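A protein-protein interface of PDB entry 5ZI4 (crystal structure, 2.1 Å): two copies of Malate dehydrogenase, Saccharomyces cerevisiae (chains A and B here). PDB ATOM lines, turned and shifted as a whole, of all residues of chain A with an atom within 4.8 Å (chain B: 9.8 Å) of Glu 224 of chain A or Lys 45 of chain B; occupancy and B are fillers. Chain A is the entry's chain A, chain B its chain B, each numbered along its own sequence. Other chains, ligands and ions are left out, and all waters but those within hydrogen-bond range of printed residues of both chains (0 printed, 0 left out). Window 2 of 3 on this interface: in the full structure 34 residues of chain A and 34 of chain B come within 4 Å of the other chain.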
ATOM      1  N   PHE A 158     -31.152 -17.599  15.992  1.00  0.00           N
ATOM      2  CA  PHE A 158     -30.084 -16.596  16.113  1.00  0.00           C
ATOM      3  C   PHE A 158     -30.525 -15.336  16.886  1.00  0.00           C
ATOM      4  O   PHE A 158     -29.648 -14.581  17.351  1.00  0.00           O
ATOM      5  CB  PHE A 158     -29.486 -16.206  14.759  1.00  0.00           C
ATOM      6  CG  PHE A 158     -28.974 -17.367  13.953  1.00  0.00           C
ATOM      7  CD1 PHE A 158     -28.507 -18.540  14.557  1.00  0.00           C
ATOM      8  CD2 PHE A 158     -28.921 -17.266  12.563  1.00  0.00           C
ATOM      9  CE1 PHE A 158     -28.010 -19.576  13.779  1.00  0.00           C
ATOM     10  CE2 PHE A 158     -28.430 -18.290  11.792  1.00  0.00           C
ATOM     11  CZ  PHE A 158     -27.994 -19.451  12.400  1.00  0.00           C
ATOM     12  N   ARG A 217     -26.265 -13.075  10.050  1.00  0.00           N
ATOM     13  CA  ARG A 217     -26.182 -14.486  10.439  1.00  0.00           C
ATOM     14  C   ARG A 217     -27.322 -15.310   9.844  1.00  0.00           C
ATOM     15  O   ARG A 217     -27.077 -16.415   9.340  1.00  0.00           O
ATOM     16  CB  ARG A 217     -26.178 -14.644  11.960  1.00  0.00           C
ATOM     17  CG  ARG A 217     -25.943 -16.077  12.428  1.00  0.00           C
ATOM     18  CD  ARG A 217     -24.669 -16.382  13.199  1.00  0.00           C
ATOM     19  NE  ARG A 217     -25.062 -16.810  14.555  1.00  0.00           N
ATOM     20  CZ  ARG A 217     -25.017 -18.046  15.043  1.00  0.00           C
ATOM     21  NH1 ARG A 217     -25.430 -18.249  16.286  1.00  0.00           N
ATOM     22  NH2 ARG A 217     -24.530 -19.066  14.340  1.00  0.00           N
ATOM     23  N   PHE A 220     -26.973 -15.476   5.963  1.00  0.00           N
ATOM     24  CA  PHE A 220     -25.892 -16.367   5.532  1.00  0.00           C
ATOM     25  C   PHE A 220     -25.754 -17.690   6.323  1.00  0.00           C
ATOM     26  O   PHE A 220     -24.678 -18.280   6.343  1.00  0.00           O
ATOM     27  CB  PHE A 220     -24.586 -15.571   5.368  1.00  0.00           C
ATOM     28  CG  PHE A 220     -24.698 -14.491   4.321  1.00  0.00           C
ATOM     29  CD1 PHE A 220     -25.339 -13.294   4.608  1.00  0.00           C
ATOM     30  CD2 PHE A 220     -24.222 -14.687   3.030  1.00  0.00           C
ATOM     31  CE1 PHE A 220     -25.473 -12.294   3.633  1.00  0.00           C
ATOM     32  CE2 PHE A 220     -24.352 -13.698   2.050  1.00  0.00           C
ATOM     33  CZ  PHE A 220     -24.988 -12.498   2.354  1.00  0.00           C
ATOM     34  N   GLY A 221     -26.877 -18.145   6.891  1.00  0.00           N
ATOM     35  CA  GLY A 221     -27.006 -19.431   7.593  1.00  0.00           C
ATOM     36  C   GLY A 221     -26.562 -20.634   6.773  1.00  0.00           C
ATOM     37  O   GLY A 221     -25.739 -21.437   7.235  1.00  0.00           O
ATOM     38  N   GLY A 222     -27.057 -20.724   5.528  1.00  0.00           N
ATOM     39  CA  GLY A 222     -26.660 -21.754   4.593  1.00  0.00           C
ATOM     40  C   GLY A 222     -25.174 -21.903   4.452  1.00  0.00           C
ATOM     41  O   GLY A 222     -24.640 -23.019   4.589  1.00  0.00           O
ATOM     42  N   ASP A 223     -24.501 -20.770   4.206  1.00  0.00           N
ATOM     43  CA  ASP A 223     -23.020 -20.715   4.098  1.00  0.00           C
ATOM     44  C   ASP A 223     -22.347 -21.223   5.338  1.00  0.00           C
ATOM     45  O   ASP A 223     -21.369 -21.954   5.256  1.00  0.00           O
ATOM     46  CB  ASP A 223     -22.508 -19.279   3.914  1.00  0.00           C
ATOM     47  CG  ASP A 223     -23.058 -18.623   2.695  1.00  0.00           C
ATOM     48  OD1 ASP A 223     -23.195 -19.320   1.673  1.00  0.00           O
ATOM     49  OD2 ASP A 223     -23.371 -17.419   2.761  1.00  0.00           O
ATOM     50  N   GLU A 224     -22.842 -20.770   6.485  1.00  0.00           N
ATOM     51  CA  GLU A 224     -22.268 -21.160   7.766  1.00  0.00           C
ATOM     52  C   GLU A 224     -22.212 -22.710   7.868  1.00  0.00           C
ATOM     53  O   GLU A 224     -21.172 -23.283   8.230  1.00  0.00           O
ATOM     54  CB  GLU A 224     -23.053 -20.498   8.897  1.00  0.00           C
ATOM     55  CG  GLU A 224     -22.709 -21.017  10.286  1.00  0.00           C
ATOM     56  CD  GLU A 224     -23.612 -20.447  11.338  1.00  0.00           C
ATOM     57  OE1 GLU A 224     -23.963 -21.168  12.320  1.00  0.00           O
ATOM     58  OE2 GLU A 224     -23.983 -19.263  11.216  1.00  0.00           O
ATOM     59  N   ILE A 225     -23.286 -23.383   7.427  1.00  0.00           N
ATOM     60  CA  ILE A 225     -23.327 -24.857   7.493  1.00  0.00           C
ATOM     61  C   ILE A 225     -22.410 -25.499   6.490  1.00  0.00           C
ATOM     62  O   ILE A 225     -21.670 -26.390   6.834  1.00  0.00           O
ATOM     63  CB  ILE A 225     -24.754 -25.403   7.395  1.00  0.00           C
ATOM     64  CG1 ILE A 225     -25.583 -24.854   8.560  1.00  0.00           C
ATOM     65  CG2 ILE A 225     -24.742 -26.939   7.423  1.00  0.00           C
ATOM     66  CD1 ILE A 225     -24.936 -25.010   9.936  1.00  0.00           C
ATOM     67  N   VAL A 226     -22.402 -24.974   5.276  1.00  0.00           N
ATOM     68  CA  VAL A 226     -21.512 -25.420   4.245  1.00  0.00           C
ATOM     69  C   VAL A 226     -20.050 -25.335   4.727  1.00  0.00           C
ATOM     70  O   VAL A 226     -19.211 -26.237   4.433  1.00  0.00           O
ATOM     71  CB  VAL A 226     -21.729 -24.559   2.951  1.00  0.00           C
ATOM     72  CG1 VAL A 226     -20.582 -24.713   1.968  1.00  0.00           C
ATOM     73  CG2 VAL A 226     -23.074 -24.879   2.292  1.00  0.00           C
ATOM     74  N   LYS A 227     -19.744 -24.256   5.445  1.00  0.00           N
ATOM     75  CA  LYS A 227     -18.387 -24.041   5.916  1.00  0.00           C
ATOM     76  C   LYS A 227     -18.068 -24.956   7.083  1.00  0.00           C
ATOM     77  O   LYS A 227     -16.971 -25.530   7.158  1.00  0.00           O
ATOM     78  CB  LYS A 227     -18.161 -22.561   6.286  1.00  0.00           C
ATOM     79  CG  LYS A 227     -18.025 -21.651   5.050  1.00  0.00           C
ATOM     80  CD  LYS A 227     -17.430 -20.288   5.393  1.00  0.00           C
ATOM     81  CE  LYS A 227     -15.893 -20.323   5.462  1.00  0.00           C
ATOM     82  NZ  LYS A 227     -15.185 -19.229   6.214  1.00  0.00           N
ATOM     83  N   ALA A 228     -19.023 -25.082   7.983  1.00  0.00           N
ATOM     84  CA  ALA A 228     -18.904 -25.957   9.131  1.00  0.00           C
ATOM     85  C   ALA A 228     -18.806 -27.416   8.686  1.00  0.00           C
ATOM     86  O   ALA A 228     -18.020 -28.158   9.255  1.00  0.00           O
ATOM     87  CB  ALA A 228     -20.091 -25.769  10.074  1.00  0.00           C
ATOM     88  N   SER B  20     -29.479 -37.951  16.543  1.00  0.00           N
ATOM     89  CA  SER B  20     -29.077 -36.631  17.012  1.00  0.00           C
ATOM     90  C   SER B  20     -30.156 -35.594  16.749  1.00  0.00           C
ATOM     91  O   SER B  20     -30.448 -34.802  17.615  1.00  0.00           O
ATOM     92  CB  SER B  20     -27.774 -36.231  16.363  1.00  0.00           C
ATOM     93  OG  SER B  20     -26.786 -37.158  16.750  1.00  0.00           O
ATOM     94  N   LYS B  24     -32.312 -33.434  19.545  1.00  0.00           N
ATOM     95  CA  LYS B  24     -32.325 -31.961  19.538  1.00  0.00           C
ATOM     96  C   LYS B  24     -33.725 -31.471  19.750  1.00  0.00           C
ATOM     97  O   LYS B  24     -33.880 -30.423  20.332  1.00  0.00           O
ATOM     98  CB  LYS B  24     -31.692 -31.324  18.272  1.00  0.00           C
ATOM     99  CG  LYS B  24     -31.700 -29.777  18.234  1.00  0.00           C
ATOM    100  CD  LYS B  24     -30.505 -29.131  18.912  1.00  0.00           C
ATOM    101  CE  LYS B  24     -30.563 -27.600  18.981  1.00  0.00           C
ATOM    102  NZ  LYS B  24     -31.820 -27.175  19.653  1.00  0.00           N
ATOM    103  N   LEU B  32     -26.538 -30.956  24.231  1.00  0.00           N
ATOM    104  CA  LEU B  32     -26.461 -32.115  23.395  1.00  0.00           C
ATOM    105  C   LEU B  32     -25.091 -32.049  22.845  1.00  0.00           C
ATOM    106  O   LEU B  32     -24.727 -31.034  22.216  1.00  0.00           O
ATOM    107  CB  LEU B  32     -27.505 -32.061  22.312  1.00  0.00           C
ATOM    108  CG  LEU B  32     -27.665 -33.323  21.432  1.00  0.00           C
ATOM    109  CD1 LEU B  32     -27.774 -34.626  22.214  1.00  0.00           C
ATOM    110  CD2 LEU B  32     -28.864 -33.176  20.510  1.00  0.00           C
ATOM    111  N   ALA B  33     -24.292 -33.087  23.104  1.00  0.00           N
ATOM    112  CA  ALA B  33     -22.955 -33.157  22.588  1.00  0.00           C
ATOM    113  C   ALA B  33     -22.851 -34.325  21.659  1.00  0.00           C
ATOM    114  O   ALA B  33     -23.243 -35.407  22.056  1.00  0.00           O
ATOM    115  CB  ALA B  33     -21.959 -33.294  23.717  1.00  0.00           C
ATOM    116  N   LEU B  34     -22.278 -34.108  20.465  1.00  0.00           N
ATOM    117  CA  LEU B  34     -22.132 -35.134  19.441  1.00  0.00           C
ATOM    118  C   LEU B  34     -20.675 -35.422  19.136  1.00  0.00           C
ATOM    119  O   LEU B  34     -19.897 -34.491  18.979  1.00  0.00           O
ATOM    120  CB  LEU B  34     -22.842 -34.678  18.173  1.00  0.00           C
ATOM    121  CG  LEU B  34     -24.255 -34.105  18.401  1.00  0.00           C
ATOM    122  CD1 LEU B  34     -24.858 -33.688  17.043  1.00  0.00           C
ATOM    123  CD2 LEU B  34     -25.147 -35.083  19.129  1.00  0.00           C
ATOM    124  N   ALA B  39     -16.837 -35.700  11.092  1.00  0.00           N
ATOM    125  CA  ALA B  39     -18.067 -34.971  10.673  1.00  0.00           C
ATOM    126  C   ALA B  39     -18.977 -34.482  11.761  1.00  0.00           C
ATOM    127  O   ALA B  39     -20.003 -33.817  11.468  1.00  0.00           O
ATOM    128  CB  ALA B  39     -18.867 -35.824   9.653  1.00  0.00           C
ATOM    129  N   ALA B  40     -18.653 -34.743  13.024  1.00  0.00           N
ATOM    130  CA  ALA B  40     -19.589 -34.398  14.057  1.00  0.00           C
ATOM    131  C   ALA B  40     -19.776 -32.888  14.254  1.00  0.00           C
ATOM    132  O   ALA B  40     -20.896 -32.437  14.526  1.00  0.00           O
ATOM    133  CB  ALA B  40     -19.265 -35.107  15.359  1.00  0.00           C
ATOM    134  N   GLU B  41     -18.712 -32.099  14.065  1.00  0.00           N
ATOM    135  CA  GLU B  41     -18.826 -30.629  14.287  1.00  0.00           C
ATOM    136  C   GLU B  41     -19.827 -29.999  13.323  1.00  0.00           C
ATOM    137  O   GLU B  41     -20.694 -29.277  13.728  1.00  0.00           O
ATOM    138  CB  GLU B  41     -17.485 -29.923  14.076  1.00  0.00           C
ATOM    139  CG  GLU B  41     -16.463 -30.229  15.144  1.00  0.00           C
ATOM    140  CD  GLU B  41     -15.030 -30.027  14.652  1.00  0.00           C
ATOM    141  OE1 GLU B  41     -14.388 -29.077  15.090  1.00  0.00           O
ATOM    142  OE2 GLU B  41     -14.539 -30.816  13.830  1.00  0.00           O
ATOM    143  N   GLY B  42     -19.705 -30.296  12.039  1.00  0.00           N
ATOM    144  CA  GLY B  42     -20.733 -29.877  11.090  1.00  0.00           C
ATOM    145  C   GLY B  42     -22.160 -30.307  11.377  1.00  0.00           C
ATOM    146  O   GLY B  42     -23.086 -29.525  11.210  1.00  0.00           O
ATOM    147  N   ILE B  43     -22.353 -31.560  11.776  1.00  0.00           N
ATOM    148  CA  ILE B  43     -23.683 -32.055  12.133  1.00  0.00           C
ATOM    149  C   ILE B  43     -24.254 -31.337  13.339  1.00  0.00           C
ATOM    150  O   ILE B  43     -25.448 -31.104  13.374  1.00  0.00           O
ATOM    151  CB  ILE B  43     -23.708 -33.601  12.348  1.00  0.00           C
ATOM    152  CG1 ILE B  43     -23.604 -34.286  10.968  1.00  0.00           C
ATOM    153  CG2 ILE B  43     -25.009 -34.073  13.030  1.00  0.00           C
ATOM    154  CD1 ILE B  43     -22.717 -35.496  10.897  1.00  0.00           C
ATOM    155  N   GLY B  44     -23.415 -31.037  14.328  1.00  0.00           N
ATOM    156  CA  GLY B  44     -23.858 -30.309  15.476  1.00  0.00           C
ATOM    157  C   GLY B  44     -24.248 -28.893  15.097  1.00  0.00           C
ATOM    158  O   GLY B  44     -25.254 -28.381  15.537  1.00  0.00           O
ATOM    159  N   LYS B  45     -23.443 -28.255  14.273  1.00  0.00           N
ATOM    160  CA  LYS B  45     -23.780 -26.921  13.821  1.00  0.00           C
ATOM    161  C   LYS B  45     -25.110 -26.880  13.077  1.00  0.00           C
ATOM    162  O   LYS B  45     -26.002 -26.045  13.353  1.00  0.00           O
ATOM    163  CB  LYS B  45     -22.613 -26.373  12.970  1.00  0.00           C
ATOM    164  CG  LYS B  45     -22.488 -24.869  13.039  1.00  0.00           C
ATOM    165  CD  LYS B  45     -21.849 -24.449  14.362  1.00  0.00           C
ATOM    166  CE  LYS B  45     -22.153 -23.008  14.635  1.00  0.00           C
ATOM    167  NZ  LYS B  45     -21.548 -22.243  13.527  1.00  0.00           N
ATOM    168  N   ASP B  46     -25.264 -27.815  12.135  1.00  0.00           N
ATOM    169  CA  ASP B  46     -26.539 -28.044  11.434  1.00  0.00           C
ATOM    170  C   ASP B  46     -27.650 -28.086  12.449  1.00  0.00           C
ATOM    171  O   ASP B  46     -28.606 -27.299  12.357  1.00  0.00           O
ATOM    172  CB  ASP B  46     -26.439 -29.321  10.568  1.00  0.00           C
ATOM    173  CG  ASP B  46     -27.715 -29.652   9.729  1.00  0.00           C
ATOM    174  OD1 ASP B  46     -28.845 -29.288  10.064  1.00  0.00           O
ATOM    175  OD2 ASP B  46     -27.531 -30.331   8.697  1.00  0.00           O
ATOM    176  N   LEU B  47     -27.565 -28.973  13.430  1.00  0.00           N
ATOM    177  CA  LEU B  47     -28.709 -29.105  14.337  1.00  0.00           C
ATOM    178  C   LEU B  47     -28.792 -27.874  15.291  1.00  0.00           C
ATOM    179  O   LEU B  47     -29.840 -27.604  15.775  1.00  0.00           O
ATOM    180  CB  LEU B  47     -28.641 -30.403  15.157  1.00  0.00           C
ATOM    181  CG  LEU B  47     -28.787 -31.771  14.449  1.00  0.00           C
ATOM    182  CD1 LEU B  47     -28.357 -32.933  15.373  1.00  0.00           C
ATOM    183  CD2 LEU B  47     -30.193 -31.958  13.978  1.00  0.00           C
ATOM    184  N   SER B  48     -27.717 -27.130  15.539  1.00  0.00           N
ATOM    185  CA  SER B  48     -27.808 -25.875  16.402  1.00  0.00           C
ATOM    186  C   SER B  48     -28.664 -24.784  15.810  1.00  0.00           C
ATOM    187  O   SER B  48     -29.159 -23.938  16.565  1.00  0.00           O
ATOM    188  CB  SER B  48     -26.474 -25.246  16.657  1.00  0.00           C
ATOM    189  OG  SER B  48     -25.894 -24.703  15.485  1.00  0.00           O
ATOM    190  N   HIS B  49     -28.879 -24.814  14.480  1.00  0.00           N
ATOM    191  CA  HIS B  49     -29.906 -23.903  13.864  1.00  0.00           C
ATOM    192  C   HIS B  49     -31.314 -24.206  14.239  1.00  0.00           C
ATOM    193  O   HIS B  49     -32.153 -23.294  14.196  1.00  0.00           O
ATOM    194  CB  HIS B  49     -29.775 -23.759  12.358  1.00  0.00           C
ATOM    195  CG  HIS B  49     -28.479 -23.155  11.961  1.00  0.00           C
ATOM    196  ND1 HIS B  49     -28.185 -22.825  10.666  1.00  0.00           N
ATOM    197  CD2 HIS B  49     -27.379 -22.847  12.691  1.00  0.00           C
ATOM    198  CE1 HIS B  49     -26.959 -22.340  10.597  1.00  0.00           C
ATOM    199  NE2 HIS B  49     -26.441 -22.357  11.815  1.00  0.00           N
ATOM    200  N   ILE B  50     -31.610 -25.422  14.705  1.00  0.00           N
ATOM    201  CA  ILE B  50     -33.008 -25.761  15.010  1.00  0.00           C
ATOM    202  C   ILE B  50     -33.491 -24.983  16.251  1.00  0.00           C
ATOM    203  O   ILE B  50     -32.822 -24.947  17.268  1.00  0.00           O
ATOM    204  CB  ILE B  50     -33.207 -27.269  15.242  1.00  0.00           C
ATOM    205  CG1 ILE B  50     -32.997 -28.078  13.958  1.00  0.00           C
ATOM    206  CG2 ILE B  50     -34.568 -27.567  15.774  1.00  0.00           C
ATOM    207  CD1 ILE B  50     -33.138 -29.579  14.146  1.00  0.00           C
ATOM    208  N   ASN B  51     -34.693 -24.438  16.177  1.00  0.00           N
ATOM    209  CA  ASN B  51     -35.220 -23.536  17.211  1.00  0.00           C
ATOM    210  C   ASN B  51     -35.853 -24.325  18.367  1.00  0.00           C
ATOM    211  O   ASN B  51     -37.044 -24.264  18.588  1.00  0.00           O
ATOM    212  CB  ASN B  51     -36.177 -22.474  16.611  1.00  0.00           C
ATOM    213  CG  ASN B  51     -37.528 -23.041  16.162  1.00  0.00           C
ATOM    214  OD1 ASN B  51     -37.608 -24.052  15.472  1.00  0.00           O
ATOM    215  ND2 ASN B  51     -38.601 -22.372  16.538  1.00  0.00           N
ATOM    216  N   SER B  54     -32.192 -26.618  23.446  1.00  0.00           N
ATOM    217  CA  SER B  54     -30.925 -27.217  23.738  1.00  0.00           C
ATOM    218  C   SER B  54     -29.724 -26.581  22.984  1.00  0.00           C
ATOM    219  O   SER B  54     -29.837 -26.114  21.853  1.00  0.00           O
ATOM    220  CB  SER B  54     -31.061 -28.719  23.444  1.00  0.00           C
ATOM    221  OG  SER B  54     -31.643 -28.985  22.176  1.00  0.00           O
ATOM    222  N   SER B  55     -28.585 -26.514  23.636  1.00  0.00           N
ATOM    223  CA  SER B  55     -27.352 -26.197  22.938  1.00  0.00           C
ATOM    224  C   SER B  55     -26.879 -27.494  22.341  1.00  0.00           C
ATOM    225  O   SER B  55     -27.050 -28.564  22.950  1.00  0.00           O
ATOM    226  CB  SER B  55     -26.321 -25.687  23.909  1.00  0.00           C
ATOM    227  OG  SER B  55     -27.029 -24.983  24.865  1.00  0.00           O
ATOM    228  N   CYS B  56     -26.297 -27.404  21.156  1.00  0.00           N
ATOM    229  CA  CYS B  56     -25.859 -28.549  20.424  1.00  0.00           C
ATOM    230  C   CYS B  56     -24.518 -28.216  19.864  1.00  0.00           C
ATOM    231  O   CYS B  56     -24.387 -27.287  19.063  1.00  0.00           O
ATOM    232  CB  CYS B  56     -26.831 -28.908  19.315  1.00  0.00           C
ATOM    233  SG  CYS B  56     -26.356 -30.469  18.530  1.00  0.00           S
ATOM    234  N   VAL B  57     -23.513 -28.956  20.316  1.00  0.00           N
ATOM    235  CA  VAL B  57     -22.159 -28.835  19.825  1.00  0.00           C
ATOM    236  C   VAL B  57     -21.754 -30.222  19.402  1.00  0.00           C
ATOM    237  O   VAL B  57     -22.076 -31.192  20.101  1.00  0.00           O
ATOM    238  CB  VAL B  57     -21.205 -28.306  20.923  1.00  0.00           C
ATOM    239  CG1 VAL B  57     -19.797 -28.169  20.379  1.00  0.00           C
ATOM    240  CG2 VAL B  57     -21.723 -26.964  21.491  1.00  0.00           C
ATOM    241  N   GLY B  58     -21.065 -30.300  18.267  1.00  0.00           N
ATOM    242  CA  GLY B  58     -20.327 -31.490  17.890  1.00  0.00           C
ATOM    243  C   GLY B  58     -18.845 -31.307  18.043  1.00  0.00           C
ATOM    244  O   GLY B  58     -18.325 -30.177  18.027  1.00  0.00           O
ATOM    245  N   TYR B  59     -18.154 -32.429  18.190  1.00  0.00           N
ATOM    246  CA  TYR B  59     -16.755 -32.422  18.553  1.00  0.00           C
ATOM    247  C   TYR B  59     -15.976 -33.252  17.603  1.00  0.00           C
ATOM    248  O   TYR B  59     -16.484 -34.229  17.053  1.00  0.00           O
ATOM    249  CB  TYR B  59     -16.566 -32.946  19.959  1.00  0.00           C
ATOM    250  CG  TYR B  59     -17.153 -32.041  20.961  1.00  0.00           C
ATOM    251  CD1 TYR B  59     -18.498 -32.136  21.312  1.00  0.00           C
ATOM    252  CD2 TYR B  59     -16.366 -31.010  21.552  1.00  0.00           C
ATOM    253  CE1 TYR B  59     -19.047 -31.251  22.226  1.00  0.00           C
ATOM    254  CE2 TYR B  59     -16.927 -30.111  22.457  1.00  0.00           C
ATOM    255  CZ  TYR B  59     -18.250 -30.237  22.767  1.00  0.00           C
ATOM    256  OH  TYR B  59     -18.791 -29.408  23.664  1.00  0.00           O
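OE1 of Glu 224 of chain A lies within salt-bridge range of NH2 of Arg 217 of chain A (3.0 Å).
The backbone carbonyl oxygen of Lys 45 of chain B is in hydrogen-bond range of the side-chain hydroxyl of Ser 48 of chain B, 2.5 Å away.
Among the printed residues, merely in contact across the chains: Phe 158 of chain A with His 49 of chain B (3.3 Å), Ile 225 of chain A with His 49 of chain B (3.4 Å), Ile 225 of chain A with Asp 46 of chain B (3.6 Å), Ile 225 of chain A with Lys 45 of chain B (3.7 Å), Gly 221 of chain A with His 49 of chain B (3.7 Å), Ala 228 of chain A with Gly 42 of chain B (3.7 Å) and Ala 228 of chain A with Lys 45 of chain B (3.9 Å).
No position is printed for both chains.
Printed residues of chain B within 4 Å of Phe 158 of chain A: His 49.
No residue of chain B comes within 4 Å of Asp 223 of chain A.
Of chain B, only Lys 45, Asp 46 and His 49 come within 4 Å of Ile 225 of chain A.
Printed residues of chain B within 4 Å of Ala 228 of chain A: Gly 42 (3.7 Å) and Lys 45 (3.9 Å).
Leu 32 of chain B touches none of the printed residues of chain A.
Of the printed residues of chain A, His 49 of chain B touches Phe 158, Gly 221, Glu 224 and Ile 225.
The side-chain amino group of Lys 45 of chain B is in salt-bridge range of the side-chain carboxylate of Glu 224 of chain A (2.9 Å).
The side-chain carboxylate (OE1) of Glu 224 of chain A lies within hydrogen-bond range of a ring nitrogen (NE2) of His 49 of chain B.
Printed residues of chain B that touch a printed residue of chain A: Gly 42, Lys 45, Asp 46 and His 49.
Hydrophobic or aromatic side chains of chain B within 4 Å of the printed part of chain A: His 49.
Hydrophobic or aromatic side chains of chain A that line the printed part of chain B: Phe 158, Ile 225 and Ala 228.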
